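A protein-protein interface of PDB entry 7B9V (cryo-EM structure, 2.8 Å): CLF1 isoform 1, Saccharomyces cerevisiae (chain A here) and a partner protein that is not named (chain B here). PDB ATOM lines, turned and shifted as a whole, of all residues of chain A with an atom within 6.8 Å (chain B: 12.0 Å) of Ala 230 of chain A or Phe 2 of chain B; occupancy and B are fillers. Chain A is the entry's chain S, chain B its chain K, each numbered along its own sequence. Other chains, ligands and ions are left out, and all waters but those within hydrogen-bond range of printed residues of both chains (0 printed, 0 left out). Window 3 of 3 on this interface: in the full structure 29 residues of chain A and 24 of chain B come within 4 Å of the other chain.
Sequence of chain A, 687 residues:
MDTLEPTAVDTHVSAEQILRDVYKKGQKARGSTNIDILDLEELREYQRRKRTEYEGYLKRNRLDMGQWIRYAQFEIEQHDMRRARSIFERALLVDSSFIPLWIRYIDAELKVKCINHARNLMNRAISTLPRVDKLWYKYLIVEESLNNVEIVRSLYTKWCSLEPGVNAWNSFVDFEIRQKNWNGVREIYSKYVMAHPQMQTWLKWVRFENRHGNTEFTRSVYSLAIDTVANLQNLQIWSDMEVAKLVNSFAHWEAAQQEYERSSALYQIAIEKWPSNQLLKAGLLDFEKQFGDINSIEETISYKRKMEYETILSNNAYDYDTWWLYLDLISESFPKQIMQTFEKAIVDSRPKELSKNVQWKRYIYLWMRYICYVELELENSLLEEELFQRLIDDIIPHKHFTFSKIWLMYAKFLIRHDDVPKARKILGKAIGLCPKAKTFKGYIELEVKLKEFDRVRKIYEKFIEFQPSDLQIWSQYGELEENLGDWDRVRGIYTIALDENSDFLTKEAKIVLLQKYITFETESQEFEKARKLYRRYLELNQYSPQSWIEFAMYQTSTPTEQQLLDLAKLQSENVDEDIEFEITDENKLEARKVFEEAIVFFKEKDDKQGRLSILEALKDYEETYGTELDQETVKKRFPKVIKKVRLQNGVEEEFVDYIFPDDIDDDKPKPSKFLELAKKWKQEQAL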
ATOM      1  N   SER A 223      24.937   7.233  -1.187  1.00  0.00           N
ATOM      2  CA  SER A 223      25.031   6.227  -0.139  1.00  0.00           C
ATOM      3  C   SER A 223      24.031   5.105  -0.381  1.00  0.00           C
ATOM      4  O   SER A 223      24.303   3.944  -0.066  1.00  0.00           O
ATOM      5  CB  SER A 223      24.846   6.883   1.223  1.00  0.00           C
ATOM      6  OG  SER A 223      23.506   7.244   1.417  1.00  0.00           O
ATOM      7  N   ALA A 225      22.998   4.162  -3.311  1.00  0.00           N
ATOM      8  CA  ALA A 225      23.538   3.390  -4.430  1.00  0.00           C
ATOM      9  C   ALA A 225      24.550   2.345  -3.960  1.00  0.00           C
ATOM     10  O   ALA A 225      24.487   1.173  -4.372  1.00  0.00           O
ATOM     11  CB  ALA A 225      24.150   4.338  -5.457  1.00  0.00           C
ATOM     12  N   ILE A 226      25.528   2.779  -3.140  1.00  0.00           N
ATOM     13  CA  ILE A 226      26.537   1.826  -2.659  1.00  0.00           C
ATOM     14  C   ILE A 226      25.903   0.782  -1.730  1.00  0.00           C
ATOM     15  O   ILE A 226      26.354  -0.379  -1.695  1.00  0.00           O
ATOM     16  CB  ILE A 226      27.762   2.494  -1.999  1.00  0.00           C
ATOM     17  CG1 ILE A 226      27.372   3.433  -0.882  1.00  0.00           C
ATOM     18  CG2 ILE A 226      28.582   3.253  -3.028  1.00  0.00           C
ATOM     19  CD1 ILE A 226      28.517   3.858  -0.028  1.00  0.00           C
ATOM     20  N   ASP A 227      24.880   1.189  -0.942  1.00  0.00           N
ATOM     21  CA  ASP A 227      24.126   0.250  -0.111  1.00  0.00           C
ATOM     22  C   ASP A 227      23.495  -0.844  -0.953  1.00  0.00           C
ATOM     23  O   ASP A 227      23.546  -2.026  -0.593  1.00  0.00           O
ATOM     24  CB  ASP A 227      23.024   0.977   0.668  1.00  0.00           C
ATOM     25  CG  ASP A 227      23.527   1.682   1.910  1.00  0.00           C
ATOM     26  OD1 ASP A 227      24.657   1.408   2.334  1.00  0.00           O
ATOM     27  OD2 ASP A 227      22.782   2.515   2.472  1.00  0.00           O
ATOM     28  N   THR A 228      22.852  -0.448  -2.058  1.00  0.00           N
ATOM     29  CA  THR A 228      22.145  -1.415  -2.884  1.00  0.00           C
ATOM     30  C   THR A 228      23.106  -2.367  -3.577  1.00  0.00           C
ATOM     31  O   THR A 228      22.796  -3.554  -3.722  1.00  0.00           O
ATOM     32  CB  THR A 228      21.260  -0.703  -3.905  1.00  0.00           C
ATOM     33  OG1 THR A 228      22.001   0.343  -4.542  1.00  0.00           O
ATOM     34  CG2 THR A 228      20.018  -0.133  -3.234  1.00  0.00           C
ATOM     35  N   VAL A 229      24.247  -1.853  -4.072  1.00  0.00           N
ATOM     36  CA  VAL A 229      25.189  -2.770  -4.722  1.00  0.00           C
ATOM     37  C   VAL A 229      25.827  -3.720  -3.721  1.00  0.00           C
ATOM     38  O   VAL A 229      26.208  -4.838  -4.087  1.00  0.00           O
ATOM     39  CB  VAL A 229      26.252  -2.050  -5.578  1.00  0.00           C
ATOM     40  CG1 VAL A 229      25.568  -1.272  -6.630  1.00  0.00           C
ATOM     41  CG2 VAL A 229      27.203  -1.173  -4.774  1.00  0.00           C
ATOM     42  N   ALA A 230      25.993  -3.296  -2.462  1.00  0.00           N
ATOM     43  CA  ALA A 230      26.502  -4.239  -1.478  1.00  0.00           C
ATOM     44  C   ALA A 230      25.465  -5.291  -1.114  1.00  0.00           C
ATOM     45  O   ALA A 230      25.767  -6.489  -1.105  1.00  0.00           O
ATOM     46  CB  ALA A 230      26.944  -3.489  -0.232  1.00  0.00           C
ATOM     47  N   ASN A 231      24.241  -4.850  -0.769  1.00  0.00           N
ATOM     48  CA  ASN A 231      23.220  -5.772  -0.279  1.00  0.00           C
ATOM     49  C   ASN A 231      22.718  -6.756  -1.333  1.00  0.00           C
ATOM     50  O   ASN A 231      22.218  -7.828  -0.975  1.00  0.00           O
ATOM     51  CB  ASN A 231      22.037  -4.971   0.270  1.00  0.00           C
ATOM     52  CG  ASN A 231      22.300  -4.414   1.661  1.00  0.00           C
ATOM     53  OD1 ASN A 231      22.509  -3.212   1.837  1.00  0.00           O
ATOM     54  ND2 ASN A 231      22.298  -5.288   2.655  1.00  0.00           N
ATOM     55  N   LEU A 232      22.840  -6.409  -2.614  1.00  0.00           N
ATOM     56  CA  LEU A 232      22.384  -7.225  -3.730  1.00  0.00           C
ATOM     57  C   LEU A 232      23.554  -7.792  -4.520  1.00  0.00           C
ATOM     58  O   LEU A 232      23.415  -8.006  -5.727  1.00  0.00           O
ATOM     59  CB  LEU A 232      21.488  -6.418  -4.662  1.00  0.00           C
ATOM     60  CG  LEU A 232      20.225  -5.805  -4.069  1.00  0.00           C
ATOM     61  CD1 LEU A 232      19.625  -4.822  -5.053  1.00  0.00           C
ATOM     62  CD2 LEU A 232      19.234  -6.890  -3.710  1.00  0.00           C
ATOM     63  N   GLN A 233      24.722  -7.943  -3.877  1.00  0.00           N
ATOM     64  CA  GLN A 233      25.922  -8.371  -4.595  1.00  0.00           C
ATOM     65  C   GLN A 233      25.779  -9.778  -5.186  1.00  0.00           C
ATOM     66  O   GLN A 233      26.180 -10.019  -6.334  1.00  0.00           O
ATOM     67  CB  GLN A 233      27.150  -8.300  -3.676  1.00  0.00           C
ATOM     68  CG  GLN A 233      28.437  -9.052  -4.137  1.00  0.00           C
ATOM     69  CD  GLN A 233      28.983  -8.756  -5.569  1.00  0.00           C
ATOM     70  OE1 GLN A 233      28.605  -7.792  -6.248  1.00  0.00           O
ATOM     71  NE2 GLN A 233      29.867  -9.639  -6.034  1.00  0.00           N
ATOM     72  N   ASN A 234      25.200 -10.719  -4.421  1.00  0.00           N
ATOM     73  CA  ASN A 234      25.096 -12.122  -4.833  1.00  0.00           C
ATOM     74  C   ASN A 234      24.163 -12.335  -6.027  1.00  0.00           C
ATOM     75  O   ASN A 234      24.186 -13.419  -6.619  1.00  0.00           O
ATOM     76  CB  ASN A 234      24.633 -13.001  -3.661  1.00  0.00           C
ATOM     77  CG  ASN A 234      23.327 -12.534  -3.054  1.00  0.00           C
ATOM     78  OD1 ASN A 234      23.229 -11.421  -2.541  1.00  0.00           O
ATOM     79  ND2 ASN A 234      22.313 -13.392  -3.100  1.00  0.00           N
ATOM     80  N   TRP A 238      25.519  -6.018 -11.543  1.00  0.00           N
ATOM     81  CA  TRP A 238      26.438  -5.027 -12.082  1.00  0.00           C
ATOM     82  C   TRP A 238      27.795  -5.653 -12.361  1.00  0.00           C
ATOM     83  O   TRP A 238      28.226  -6.582 -11.673  1.00  0.00           O
ATOM     84  CB  TRP A 238      26.625  -3.849 -11.124  1.00  0.00           C
ATOM     85  CG  TRP A 238      25.359  -3.240 -10.674  1.00  0.00           C
ATOM     86  CD1 TRP A 238      24.696  -2.204 -11.254  1.00  0.00           C
ATOM     87  CD2 TRP A 238      24.587  -3.630  -9.539  1.00  0.00           C
ATOM     88  NE1 TRP A 238      23.558  -1.915 -10.542  1.00  0.00           N
ATOM     89  CE2 TRP A 238      23.467  -2.780  -9.484  1.00  0.00           C
ATOM     90  CE3 TRP A 238      24.735  -4.616  -8.559  1.00  0.00           C
ATOM     91  CZ2 TRP A 238      22.500  -2.884  -8.489  1.00  0.00           C
ATOM     92  CZ3 TRP A 238      23.774  -4.721  -7.574  1.00  0.00           C
ATOM     93  CH2 TRP A 238      22.671  -3.859  -7.544  1.00  0.00           C
ATOM     94  N   VAL A 247      31.589   3.789  -6.971  1.00  0.00           N
ATOM     95  CA  VAL A 247      32.279   4.160  -5.736  1.00  0.00           C
ATOM     96  C   VAL A 247      33.403   5.170  -6.018  1.00  0.00           C
ATOM     97  O   VAL A 247      33.706   6.021  -5.164  1.00  0.00           O
ATOM     98  CB  VAL A 247      32.692   2.865  -4.993  1.00  0.00           C
ATOM     99  CG1 VAL A 247      33.636   2.102  -5.776  1.00  0.00           C
ATOM    100  CG2 VAL A 247      33.321   3.163  -3.624  1.00  0.00           C
ATOM    101  N   LEU A 266      35.866   5.313   2.465  1.00  0.00           N
ATOM    102  CA  LEU A 266      34.952   4.622   1.555  1.00  0.00           C
ATOM    103  C   LEU A 266      35.664   3.593   0.696  1.00  0.00           C
ATOM    104  O   LEU A 266      35.141   2.493   0.458  1.00  0.00           O
ATOM    105  CB  LEU A 266      34.266   5.652   0.677  1.00  0.00           C
ATOM    106  CG  LEU A 266      33.369   5.206  -0.462  1.00  0.00           C
ATOM    107  CD1 LEU A 266      32.224   4.323   0.019  1.00  0.00           C
ATOM    108  CD2 LEU A 266      32.881   6.457  -1.141  1.00  0.00           C
ATOM    109  N   GLN A 268      38.405   2.039   1.566  1.00  0.00           N
ATOM    110  CA  GLN A 268      38.816   0.944   2.445  1.00  0.00           C
ATOM    111  C   GLN A 268      37.690  -0.068   2.631  1.00  0.00           C
ATOM    112  O   GLN A 268      37.918  -1.284   2.542  1.00  0.00           O
ATOM    113  CB  GLN A 268      39.295   1.480   3.800  1.00  0.00           C
ATOM    114  CG  GLN A 268      39.701   0.422   4.843  1.00  0.00           C
ATOM    115  CD  GLN A 268      40.782  -0.561   4.381  1.00  0.00           C
ATOM    116  OE1 GLN A 268      41.625  -0.257   3.530  1.00  0.00           O
ATOM    117  NE2 GLN A 268      40.742  -1.763   4.941  1.00  0.00           N
ATOM    118  N   ILE A 269      36.470   0.428   2.917  1.00  0.00           N
ATOM    119  CA  ILE A 269      35.330  -0.485   3.094  1.00  0.00           C
ATOM    120  C   ILE A 269      35.023  -1.205   1.771  1.00  0.00           C
ATOM    121  O   ILE A 269      34.719  -2.413   1.759  1.00  0.00           O
ATOM    122  CB  ILE A 269      34.086   0.200   3.723  1.00  0.00           C
ATOM    123  CG1 ILE A 269      34.268   0.648   5.189  1.00  0.00           C
ATOM    124  CG2 ILE A 269      32.943  -0.752   3.882  1.00  0.00           C
ATOM    125  CD1 ILE A 269      34.901   1.944   5.519  1.00  0.00           C
ATOM    126  N   ALA A 270      35.089  -0.472   0.641  1.00  0.00           N
ATOM    127  CA  ALA A 270      34.830  -1.082  -0.664  1.00  0.00           C
ATOM    128  C   ALA A 270      35.853  -2.170  -0.997  1.00  0.00           C
ATOM    129  O   ALA A 270      35.494  -3.205  -1.570  1.00  0.00           O
ATOM    130  CB  ALA A 270      34.816  -0.009  -1.749  1.00  0.00           C
ATOM    131  N   ILE A 271      37.138  -1.930  -0.682  1.00  0.00           N
ATOM    132  CA  ILE A 271      38.180  -2.925  -0.935  1.00  0.00           C
ATOM    133  C   ILE A 271      37.959  -4.154  -0.058  1.00  0.00           C
ATOM    134  O   ILE A 271      38.166  -5.293  -0.508  1.00  0.00           O
ATOM    135  CB  ILE A 271      39.589  -2.298  -0.755  1.00  0.00           C
ATOM    136  CG1 ILE A 271      39.915  -1.342  -1.908  1.00  0.00           C
ATOM    137  CG2 ILE A 271      40.728  -3.329  -0.545  1.00  0.00           C
ATOM    138  CD1 ILE A 271      40.350  -2.004  -3.168  1.00  0.00           C
ATOM    139  N   LYS A 273      35.076  -5.225   0.811  1.00  0.00           N
ATOM    140  CA  LYS A 273      33.910  -5.933   0.297  1.00  0.00           C
ATOM    141  C   LYS A 273      34.193  -6.639  -1.027  1.00  0.00           C
ATOM    142  O   LYS A 273      33.662  -7.727  -1.271  1.00  0.00           O
ATOM    143  CB  LYS A 273      32.731  -4.977   0.136  1.00  0.00           C
ATOM    144  CG  LYS A 273      31.391  -5.683   0.186  1.00  0.00           C
ATOM    145  CD  LYS A 273      30.894  -5.823   1.611  1.00  0.00           C
ATOM    146  CE  LYS A 273      29.605  -6.624   1.666  1.00  0.00           C
ATOM    147  NZ  LYS A 273      29.830  -8.077   1.426  1.00  0.00           N
ATOM    148  N   TRP A 274      35.031  -6.044  -1.878  1.00  0.00           N
ATOM    149  CA  TRP A 274      35.222  -6.486  -3.263  1.00  0.00           C
ATOM    150  C   TRP A 274      36.707  -6.689  -3.546  1.00  0.00           C
ATOM    151  O   TRP A 274      37.334  -5.847  -4.202  1.00  0.00           O
ATOM    152  CB  TRP A 274      34.619  -5.479  -4.245  1.00  0.00           C
ATOM    153  CG  TRP A 274      33.135  -5.349  -4.128  1.00  0.00           C
ATOM    154  CD1 TRP A 274      32.203  -6.301  -4.408  1.00  0.00           C
ATOM    155  CD2 TRP A 274      32.412  -4.191  -3.697  1.00  0.00           C
ATOM    156  NE1 TRP A 274      30.942  -5.811  -4.172  1.00  0.00           N
ATOM    157  CE2 TRP A 274      31.044  -4.516  -3.736  1.00  0.00           C
ATOM    158  CE3 TRP A 274      32.789  -2.911  -3.284  1.00  0.00           C
ATOM    159  CZ2 TRP A 274      30.051  -3.608  -3.374  1.00  0.00           C
ATOM    160  CZ3 TRP A 274      31.806  -2.012  -2.924  1.00  0.00           C
ATOM    161  CH2 TRP A 274      30.452  -2.364  -2.972  1.00  0.00           C
ATOM    162  N   MET B   1      23.415  -0.499   5.924  1.00  0.00           N
ATOM    163  CA  MET B   1      24.580  -1.178   6.480  1.00  0.00           C
ATOM    164  C   MET B   1      25.852  -0.460   6.064  1.00  0.00           C
ATOM    165  O   MET B   1      26.590   0.017   6.926  1.00  0.00           O
ATOM    166  CB  MET B   1      24.618  -2.645   6.028  1.00  0.00           C
ATOM    167  CG  MET B   1      25.589  -3.590   6.772  1.00  0.00           C
ATOM    168  SD  MET B   1      27.369  -3.498   6.436  1.00  0.00           S
ATOM    169  CE  MET B   1      27.420  -4.143   4.765  1.00  0.00           C
ATOM    170  N   PHE B   2      26.117  -0.476   4.748  1.00  0.00           N
ATOM    171  CA  PHE B   2      27.381   0.014   4.190  1.00  0.00           C
ATOM    172  C   PHE B   2      27.581   1.495   4.474  1.00  0.00           C
ATOM    173  O   PHE B   2      28.705   1.922   4.772  1.00  0.00           O
ATOM    174  CB  PHE B   2      27.401  -0.283   2.679  1.00  0.00           C
ATOM    175  CG  PHE B   2      28.779  -0.299   2.018  1.00  0.00           C
ATOM    176  CD1 PHE B   2      29.518   0.872   1.842  1.00  0.00           C
ATOM    177  CD2 PHE B   2      29.312  -1.484   1.545  1.00  0.00           C
ATOM    178  CE1 PHE B   2      30.744   0.858   1.211  1.00  0.00           C
ATOM    179  CE2 PHE B   2      30.543  -1.508   0.914  1.00  0.00           C
ATOM    180  CZ  PHE B   2      31.261  -0.338   0.754  1.00  0.00           C
ATOM    181  N   SER B   3      26.517   2.299   4.345  1.00  0.00           N
ATOM    182  CA  SER B   3      26.647   3.735   4.563  1.00  0.00           C
ATOM    183  C   SER B   3      26.949   4.065   6.021  1.00  0.00           C
ATOM    184  O   SER B   3      27.549   5.106   6.306  1.00  0.00           O
ATOM    185  CB  SER B   3      25.374   4.444   4.106  1.00  0.00           C
ATOM    186  OG  SER B   3      24.244   3.925   4.784  1.00  0.00           O
ATOM    187  N   ASN B   4      26.547   3.191   6.951  1.00  0.00           N
ATOM    188  CA  ASN B   4      26.830   3.418   8.361  1.00  0.00           C
ATOM    189  C   ASN B   4      28.301   3.212   8.709  1.00  0.00           C
ATOM    190  O   ASN B   4      28.759   3.739   9.727  1.00  0.00           O
ATOM    191  CB  ASN B   4      25.972   2.491   9.220  1.00  0.00           C
ATOM    192  CG  ASN B   4      24.494   2.805   9.119  1.00  0.00           C
ATOM    193  OD1 ASN B   4      23.835   2.439   8.146  1.00  0.00           O
ATOM    194  ND2 ASN B   4      23.963   3.484  10.128  1.00  0.00           N
ATOM    195  N   ARG B   5      29.043   2.447   7.899  1.00  0.00           N
ATOM    196  CA  ARG B   5      30.457   2.204   8.173  1.00  0.00           C
ATOM    197  C   ARG B   5      31.331   3.429   7.929  1.00  0.00           C
ATOM    198  O   ARG B   5      32.450   3.486   8.447  1.00  0.00           O
ATOM    199  CB  ARG B   5      30.957   1.023   7.336  1.00  0.00           C
ATOM    200  CG  ARG B   5      30.333  -0.317   7.720  1.00  0.00           C
ATOM    201  CD  ARG B   5      31.074  -1.496   7.108  1.00  0.00           C
ATOM    202  NE  ARG B   5      32.430  -1.628   7.627  1.00  0.00           N
ATOM    203  CZ  ARG B   5      33.320  -2.503   7.182  1.00  0.00           C
ATOM    204  NH1 ARG B   5      33.029  -3.348   6.208  1.00  0.00           N
ATOM    205  NH2 ARG B   5      34.530  -2.535   7.731  1.00  0.00           N
ATOM    206  N   LEU B   6      30.846   4.410   7.157  1.00  0.00           N
ATOM    207  CA  LEU B   6      31.644   5.583   6.847  1.00  0.00           C
ATOM    208  C   LEU B   6      31.608   6.568   8.017  1.00  0.00           C
ATOM    209  O   LEU B   6      30.634   6.589   8.774  1.00  0.00           O
ATOM    210  CB  LEU B   6      31.103   6.259   5.584  1.00  0.00           C
ATOM    211  CG  LEU B   6      30.848   5.377   4.368  1.00  0.00           C
ATOM    212  CD1 LEU B   6      30.218   6.183   3.240  1.00  0.00           C
ATOM    213  CD2 LEU B   6      32.115   4.700   3.934  1.00  0.00           C
ATOM    214  N   PRO B   7      32.652   7.380   8.208  1.00  0.00           N
ATOM    215  CA  PRO B   7      32.618   8.378   9.286  1.00  0.00           C
ATOM    216  C   PRO B   7      31.662   9.509   8.941  1.00  0.00           C
ATOM    217  O   PRO B   7      31.327   9.682   7.762  1.00  0.00           O
ATOM    218  CB  PRO B   7      34.077   8.865   9.355  1.00  0.00           C
ATOM    219  CG  PRO B   7      34.594   8.676   7.998  1.00  0.00           C
ATOM    220  CD  PRO B   7      33.938   7.429   7.482  1.00  0.00           C
ATOM    221  N   PRO B   8      31.141  10.252   9.929  1.00  0.00           N
ATOM    222  CA  PRO B   8      30.200  11.329   9.612  1.00  0.00           C
ATOM    223  C   PRO B   8      30.908  12.494   8.940  1.00  0.00           C
ATOM    224  O   PRO B   8      32.125  12.675   9.118  1.00  0.00           O
ATOM    225  CB  PRO B   8      29.637  11.723  10.989  1.00  0.00           C
ATOM    226  CG  PRO B   8      30.694  11.372  11.936  1.00  0.00           C
ATOM    227  CD  PRO B   8      31.365  10.144  11.386  1.00  0.00           C
ATOM    228  N   PRO B   9      30.204  13.280   8.120  1.00  0.00           N
ATOM    229  CA  PRO B   9      30.837  14.467   7.532  1.00  0.00           C
ATOM    230  C   PRO B   9      31.117  15.537   8.579  1.00  0.00           C
ATOM    231  O   PRO B   9      30.377  15.704   9.551  1.00  0.00           O
ATOM    232  CB  PRO B   9      29.807  14.945   6.501  1.00  0.00           C
ATOM    233  CG  PRO B   9      28.505  14.464   7.030  1.00  0.00           C
ATOM    234  CD  PRO B   9      28.800  13.142   7.686  1.00  0.00           C
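The backbone NH of Phe 2 of chain B sits close to the side-chain carboxylate of Asp 227 of chain A (3.4 Å). The side-chain carboxylate (OD1) of Asp 227 of chain A lies within hydrogen-bond range of the backbone NH (N) of Ser 3 of chain B (2.9 Å).
The side-chain amide oxygen (OD1) of Asn 231 of chain A sits close to the backbone carbonyl oxygen (O) of Asp 227 of chain A, at 2.9 Å.
Among the printed residues, pairs that only touch across the chains: Ser 223 of chain A with Ser 3 of chain B (3.8 Å), Ile 226 of chain A with Phe 2 of chain B (3.7 Å), Ala 230 of chain A with Phe 2 of chain B (3.6 Å), Leu 266 of chain A with Phe 2 of chain B (3.95 Å), Leu 266 of chain A with Leu 6 of chain B (3.7 Å), Ile 269 of chain A with Phe 2 of chain B (3.6 Å), Ile 269 of chain A with Arg 5 of chain B (3.5 Å), Ala 270 of chain A with Phe 2 of chain B (3.8 Å) and Trp 274 of chain A with Phe 2 of chain B (3.98 Å).
Ala 230 of chain A touches one residue of chain B. Of the printed residues of chain A, Phe 2 of chain B touches Ile 226 (3.7 Å), Asp 227 (3.2 Å), Ala 230 (3.6 Å), Leu 266 (3.95 Å), Ile 269 (3.6 Å), Ala 270 (3.8 Å) and Trp 274 (3.98 Å). Ile 226 of chain A touches one residue of chain B. Printed residues of chain B within 4 Å of Asp 227 of chain A: Phe 2 (3.2 Å) and Ser 3 (2.9 Å). No residue of chain B comes within 4 Å of Thr 228 of chain A. Val 229 of chain A touches none of the printed residues of chain B. No residue of chain B comes within 4 Å of Asn 231 of chain A. No residue of chain B comes within 4 Å of Leu 232 of chain A. No residue of chain B comes within 4 Å of Gln 233 of chain A. Leu 266 of chain A touches two residues of chain B. Printed residues of chain B within 4 Å of Ala 270 of chain A: Phe 2 (3.8 Å). Printed residues of chain A within 4 Å of Arg 5 of chain B: Ile 269 (3.5 Å). Of the printed residues of chain B, Ser 223 of chain A touches Ser 3. Pro 9 of chain B touches none of the printed residues of chain A. Ile 271 of chain A touches none of the printed residues of chain B. The nearest printed residue of chain A that does not touch Phe 2 of chain B is Lys 273 of chain A (4.2 Å).
Of the 20 printed residues of chain A, 8 touch a printed residue of chain B. Hydrophobic or aromatic side chains of chain A that line the printed part of chain B: Ile 226, Ala 230, Leu 266, Ile 269 and Trp 274. Of the 9 printed residues of chain B, 4 touch a printed residue of chain A. Hydrophobic or aromatic side chains of chain B that line the printed part of chain A: Phe 2 and Leu 6. Along chain B the printed residues that touch a printed residue of chain A span positions 2 to 6. Among the printed residues, 11 pairs touch across the chains.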
